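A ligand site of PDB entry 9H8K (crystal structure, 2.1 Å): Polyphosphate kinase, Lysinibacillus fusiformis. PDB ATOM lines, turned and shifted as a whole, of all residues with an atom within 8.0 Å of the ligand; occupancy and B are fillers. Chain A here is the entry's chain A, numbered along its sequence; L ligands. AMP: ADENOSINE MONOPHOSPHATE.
NE1 of Trp 183 lies within hydrogen-bond range of N1 of the ligand, 3.4 Å away.
The side-chain amino group (NZ) of Lys 166 sits at hydrogen-bond distance from an oxygen (O3') of the ligand (3.0 Å).
OD1 of Asp 180 sits at hydrogen-bond distance from N6 of the ligand (3.5 Å).
Residues that only touch the ligand: Leu 162 (3.96 Å) and Glu 169 (3.2 Å).
Within 4 Å of the ligand: Leu 162, Lys 166, Glu 169, Asp 180 and Trp 183.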
ATOM      1  N   LEU A 162      29.127   1.952  -5.735  1.00  0.00           N
ATOM      2  CA  LEU A 162      29.656   1.312  -6.942  1.00  0.00           C
ATOM      3  C   LEU A 162      31.094   1.765  -7.211  1.00  0.00           C
ATOM      4  O   LEU A 162      31.972   0.957  -7.555  1.00  0.00           O
ATOM      5  CB  LEU A 162      28.765   1.600  -8.157  1.00  0.00           C
ATOM      6  CG  LEU A 162      29.184   0.951  -9.491  1.00  0.00           C
ATOM      7  CD1 LEU A 162      29.083  -0.552  -9.415  1.00  0.00           C
ATOM      8  CD2 LEU A 162      28.386   1.476 -10.713  1.00  0.00           C
ATOM      9  N   LYS A 163      31.338   3.069  -7.068  1.00  0.00           N
ATOM     10  CA  LYS A 163      32.708   3.573  -7.187  1.00  0.00           C
ATOM     11  C   LYS A 163      33.648   2.839  -6.228  1.00  0.00           C
ATOM     12  O   LYS A 163      34.757   2.424  -6.611  1.00  0.00           O
ATOM     13  CB  LYS A 163      32.716   5.083  -6.918  1.00  0.00           C
ATOM     14  CG  LYS A 163      34.083   5.726  -6.963  1.00  0.00           C
ATOM     15  CD  LYS A 163      33.970   7.228  -6.671  1.00  0.00           C
ATOM     16  CE  LYS A 163      35.330   7.891  -6.652  1.00  0.00           C
ATOM     17  NZ  LYS A 163      35.303   9.142  -5.846  1.00  0.00           N
ATOM     18  N   PHE A 165      33.227  -0.173  -4.824  1.00  0.00           N
ATOM     19  CA  PHE A 165      33.353  -1.554  -5.254  1.00  0.00           C
ATOM     20  C   PHE A 165      34.407  -1.684  -6.342  1.00  0.00           C
ATOM     21  O   PHE A 165      35.215  -2.620  -6.339  1.00  0.00           O
ATOM     22  CB  PHE A 165      32.006  -2.092  -5.757  1.00  0.00           C
ATOM     23  CG  PHE A 165      31.117  -2.694  -4.693  1.00  0.00           C
ATOM     24  CD1 PHE A 165      31.060  -2.160  -3.400  1.00  0.00           C
ATOM     25  CD2 PHE A 165      30.306  -3.781  -4.995  1.00  0.00           C
ATOM     26  CE1 PHE A 165      30.227  -2.705  -2.450  1.00  0.00           C
ATOM     27  CE2 PHE A 165      29.476  -4.346  -4.034  1.00  0.00           C
ATOM     28  CZ  PHE A 165      29.427  -3.801  -2.762  1.00  0.00           C
ATOM     29  N   LYS A 166      34.408  -0.750  -7.295  1.00  0.00           N
ATOM     30  CA  LYS A 166      35.361  -0.839  -8.397  1.00  0.00           C
ATOM     31  C   LYS A 166      36.785  -0.552  -7.925  1.00  0.00           C
ATOM     32  O   LYS A 166      37.744  -1.215  -8.361  1.00  0.00           O
ATOM     33  CB  LYS A 166      34.940   0.118  -9.512  1.00  0.00           C
ATOM     34  CG  LYS A 166      33.635  -0.316 -10.180  1.00  0.00           C
ATOM     35  CD  LYS A 166      33.209   0.607 -11.309  1.00  0.00           C
ATOM     36  CE  LYS A 166      32.087  -0.044 -12.138  1.00  0.00           C
ATOM     37  NZ  LYS A 166      31.492   0.897 -13.122  1.00  0.00           N
ATOM     38  N   GLU A 169      37.885  -3.714  -6.303  1.00  0.00           N
ATOM     39  CA  GLU A 169      38.191  -4.683  -7.353  1.00  0.00           C
ATOM     40  C   GLU A 169      39.569  -4.455  -7.941  1.00  0.00           C
ATOM     41  O   GLU A 169      40.172  -5.411  -8.454  1.00  0.00           O
ATOM     42  CB  GLU A 169      37.109  -4.594  -8.430  1.00  0.00           C
ATOM     43  CG  GLU A 169      37.141  -5.698  -9.451  1.00  0.00           C
ATOM     44  CD  GLU A 169      36.090  -5.498 -10.521  1.00  0.00           C
ATOM     45  OE1 GLU A 169      35.837  -4.329 -10.882  1.00  0.00           O
ATOM     46  OE2 GLU A 169      35.501  -6.510 -10.981  1.00  0.00           O
ATOM     47  N   LEU A 178      36.058  -9.410  -2.538  1.00  0.00           N
ATOM     48  CA  LEU A 178      34.864  -8.943  -3.221  1.00  0.00           C
ATOM     49  C   LEU A 178      34.421 -10.027  -4.189  1.00  0.00           C
ATOM     50  O   LEU A 178      35.136 -10.325  -5.155  1.00  0.00           O
ATOM     51  CB  LEU A 178      35.152  -7.626  -3.944  1.00  0.00           C
ATOM     52  CG  LEU A 178      34.012  -6.999  -4.732  1.00  0.00           C
ATOM     53  CD1 LEU A 178      32.854  -6.637  -3.812  1.00  0.00           C
ATOM     54  CD2 LEU A 178      34.533  -5.786  -5.471  1.00  0.00           C
ATOM     55  N   THR A 179      33.271 -10.631  -3.925  1.00  0.00           N
ATOM     56  CA  THR A 179      32.778 -11.806  -4.648  1.00  0.00           C
ATOM     57  C   THR A 179      31.605 -11.434  -5.550  1.00  0.00           C
ATOM     58  O   THR A 179      31.064 -10.315  -5.476  1.00  0.00           O
ATOM     59  CB  THR A 179      32.341 -12.893  -3.661  1.00  0.00           C
ATOM     60  OG1 THR A 179      31.196 -12.441  -2.922  1.00  0.00           O
ATOM     61  CG2 THR A 179      33.462 -13.207  -2.680  1.00  0.00           C
ATOM     62  N   ASP A 180      31.218 -12.375  -6.405  1.00  0.00           N
ATOM     63  CA  ASP A 180      30.044 -12.185  -7.255  1.00  0.00           C
ATOM     64  C   ASP A 180      28.771 -11.996  -6.421  1.00  0.00           C
ATOM     65  O   ASP A 180      27.893 -11.226  -6.800  1.00  0.00           O
ATOM     66  CB  ASP A 180      29.886 -13.366  -8.212  1.00  0.00           C
ATOM     67  CG  ASP A 180      30.990 -13.410  -9.261  1.00  0.00           C
ATOM     68  OD1 ASP A 180      31.876 -12.520  -9.242  1.00  0.00           O
ATOM     69  OD2 ASP A 180      30.974 -14.317 -10.117  1.00  0.00           O
ATOM     70  N   GLU A 181      28.690 -12.669  -5.272  1.00  0.00           N
ATOM     71  CA  GLU A 181      27.532 -12.513  -4.396  1.00  0.00           C
ATOM     72  C   GLU A 181      27.467 -11.112  -3.791  1.00  0.00           C
ATOM     73  O   GLU A 181      26.373 -10.584  -3.569  1.00  0.00           O
ATOM     74  CB  GLU A 181      27.550 -13.567  -3.292  1.00  0.00           C
ATOM     75  CG  GLU A 181      26.297 -13.598  -2.440  1.00  0.00           C
ATOM     76  CD  GLU A 181      26.372 -14.603  -1.311  1.00  0.00           C
ATOM     77  OE1 GLU A 181      27.362 -15.358  -1.249  1.00  0.00           O
ATOM     78  OE2 GLU A 181      25.439 -14.632  -0.485  1.00  0.00           O
ATOM     79  N   ASP A 182      28.628 -10.490  -3.532  1.00  0.00           N
ATOM     80  CA  ASP A 182      28.615  -9.110  -3.041  1.00  0.00           C
ATOM     81  C   ASP A 182      28.032  -8.172  -4.088  1.00  0.00           C
ATOM     82  O   ASP A 182      27.264  -7.256  -3.752  1.00  0.00           O
ATOM     83  CB  ASP A 182      30.032  -8.673  -2.659  1.00  0.00           C
ATOM     84  CG  ASP A 182      30.591  -9.465  -1.485  1.00  0.00           C
ATOM     85  OD1 ASP A 182      29.818  -9.852  -0.591  1.00  0.00           O
ATOM     86  OD2 ASP A 182      31.819  -9.689  -1.475  1.00  0.00           O
ATOM     87  N   TRP A 183      28.394  -8.365  -5.353  1.00  0.00           N
ATOM     88  CA  TRP A 183      27.826  -7.554  -6.426  1.00  0.00           C
ATOM     89  C   TRP A 183      26.320  -7.795  -6.568  1.00  0.00           C
ATOM     90  O   TRP A 183      25.547  -6.849  -6.773  1.00  0.00           O
ATOM     91  CB  TRP A 183      28.518  -7.863  -7.745  1.00  0.00           C
ATOM     92  CG  TRP A 183      29.904  -7.328  -7.876  1.00  0.00           C
ATOM     93  CD1 TRP A 183      31.057  -7.999  -7.651  1.00  0.00           C
ATOM     94  CD2 TRP A 183      30.275  -6.009  -8.274  1.00  0.00           C
ATOM     95  NE1 TRP A 183      32.140  -7.178  -7.891  1.00  0.00           N
ATOM     96  CE2 TRP A 183      31.684  -5.952  -8.279  1.00  0.00           C
ATOM     97  CE3 TRP A 183      29.553  -4.865  -8.643  1.00  0.00           C
ATOM     98  CZ2 TRP A 183      32.385  -4.794  -8.618  1.00  0.00           C
ATOM     99  CZ3 TRP A 183      30.257  -3.719  -8.988  1.00  0.00           C
ATOM    100  CH2 TRP A 183      31.663  -3.699  -8.981  1.00  0.00           C
ATOM    101  N   ARG A 184      25.893  -9.066  -6.474  1.00  0.00           N
ATOM    102  CA  ARG A 184      24.469  -9.359  -6.600  1.00  0.00           C
ATOM    103  C   ARG A 184      23.666  -8.772  -5.450  1.00  0.00           C
ATOM    104  O   ARG A 184      22.500  -8.377  -5.647  1.00  0.00           O
ATOM    105  CB  ARG A 184      24.244 -10.878  -6.679  1.00  0.00           C
ATOM    106  CG  ARG A 184      24.805 -11.546  -7.916  1.00  0.00           C
ATOM    107  CD  ARG A 184      24.351 -13.000  -8.017  1.00  0.00           C
ATOM    108  NE  ARG A 184      24.540 -13.735  -6.776  1.00  0.00           N
ATOM    109  CZ  ARG A 184      25.503 -14.629  -6.570  1.00  0.00           C
ATOM    110  NH1 ARG A 184      26.364 -14.946  -7.514  1.00  0.00           N
ATOM    111  NH2 ARG A 184      25.588 -15.225  -5.378  1.00  0.00           N
ATOM    112  N   ARG A 186      23.849  -5.984  -4.229  1.00  0.00           N
ATOM    113  CA  ARG A 186      23.503  -4.590  -4.500  1.00  0.00           C
ATOM    114  C   ARG A 186      22.072  -4.454  -5.010  1.00  0.00           C
ATOM    115  O   ARG A 186      21.457  -3.397  -4.836  1.00  0.00           O
ATOM    116  CB  ARG A 186      24.499  -3.983  -5.507  1.00  0.00           C
ATOM    117  CG  ARG A 186      25.762  -3.425  -4.840  1.00  0.00           C
ATOM    118  CD  ARG A 186      26.776  -2.921  -5.851  1.00  0.00           C
ATOM    119  NE  ARG A 186      26.166  -2.157  -6.942  1.00  0.00           N
ATOM    120  CZ  ARG A 186      25.942  -0.858  -6.917  1.00  0.00           C
ATOM    121  NH1 ARG A 186      26.249  -0.131  -5.854  1.00  0.00           N
ATOM    122  NH2 ARG A 186      25.401  -0.263  -7.976  1.00  0.00           N
ATOM    123  N   GLU A 187      21.528  -5.510  -5.630  1.00  0.00           N
ATOM    124  CA  GLU A 187      20.145  -5.500  -6.090  1.00  0.00           C
ATOM    125  C   GLU A 187      19.140  -5.498  -4.928  1.00  0.00           C
ATOM    126  O   GLU A 187      17.965  -5.191  -5.142  1.00  0.00           O
ATOM    127  CB  GLU A 187      19.883  -6.702  -6.987  1.00  0.00           C
ATOM    128  CG  GLU A 187      18.582  -6.648  -7.772  1.00  0.00           C
ATOM    129  CD  GLU A 187      18.392  -7.861  -8.661  1.00  0.00           C
ATOM    130  OE1 GLU A 187      19.331  -8.675  -8.765  1.00  0.00           O
ATOM    131  OE2 GLU A 187      17.289  -8.017  -9.251  1.00  0.00           O
HETATM  132  P   AMP L   1      24.795  -5.021 -14.248  1.00  0.00           P
HETATM  133  O1P AMP L   1      23.833  -4.239 -15.107  1.00  0.00           O
HETATM  134  O2P AMP L   1      25.295  -6.338 -14.798  1.00  0.00           O
HETATM  135  O3P AMP L   1      24.330  -5.143 -12.804  1.00  0.00           O
HETATM  136  O5' AMP L   1      26.086  -4.092 -14.173  1.00  0.00           O
HETATM  137  C5' AMP L   1      26.039  -2.863 -13.456  1.00  0.00           C
HETATM  138  C4' AMP L   1      27.364  -2.508 -12.833  1.00  0.00           C
HETATM  139  O4' AMP L   1      27.755  -3.544 -11.904  1.00  0.00           O
HETATM  140  C3' AMP L   1      28.527  -2.335 -13.814  1.00  0.00           C
HETATM  141  O3' AMP L   1      29.371  -1.267 -13.389  1.00  0.00           O
HETATM  142  C2' AMP L   1      29.265  -3.664 -13.692  1.00  0.00           C
HETATM  143  O2' AMP L   1      30.639  -3.603 -14.018  1.00  0.00           O
HETATM  144  C1' AMP L   1      29.052  -4.011 -12.221  1.00  0.00           C
HETATM  145  N9  AMP L   1      29.112  -5.444 -11.913  1.00  0.00           N
HETATM  146  C8  AMP L   1      28.060  -6.282 -11.674  1.00  0.00           C
HETATM  147  N7  AMP L   1      28.409  -7.507 -11.360  1.00  0.00           N
HETATM  148  C5  AMP L   1      29.799  -7.474 -11.392  1.00  0.00           C
HETATM  149  C6  AMP L   1      30.775  -8.446 -11.118  1.00  0.00           C
HETATM  150  N6  AMP L   1      30.500  -9.706 -10.765  1.00  0.00           N
HETATM  151  N1  AMP L   1      32.074  -8.071 -11.219  1.00  0.00           N
HETATM  152  C2  AMP L   1      32.356  -6.815 -11.561  1.00  0.00           C
HETATM  153  N3  AMP L   1      31.525  -5.812 -11.842  1.00  0.00           N
HETATM  154  C4  AMP L   1      30.241  -6.210 -11.732  1.00  0.00           C
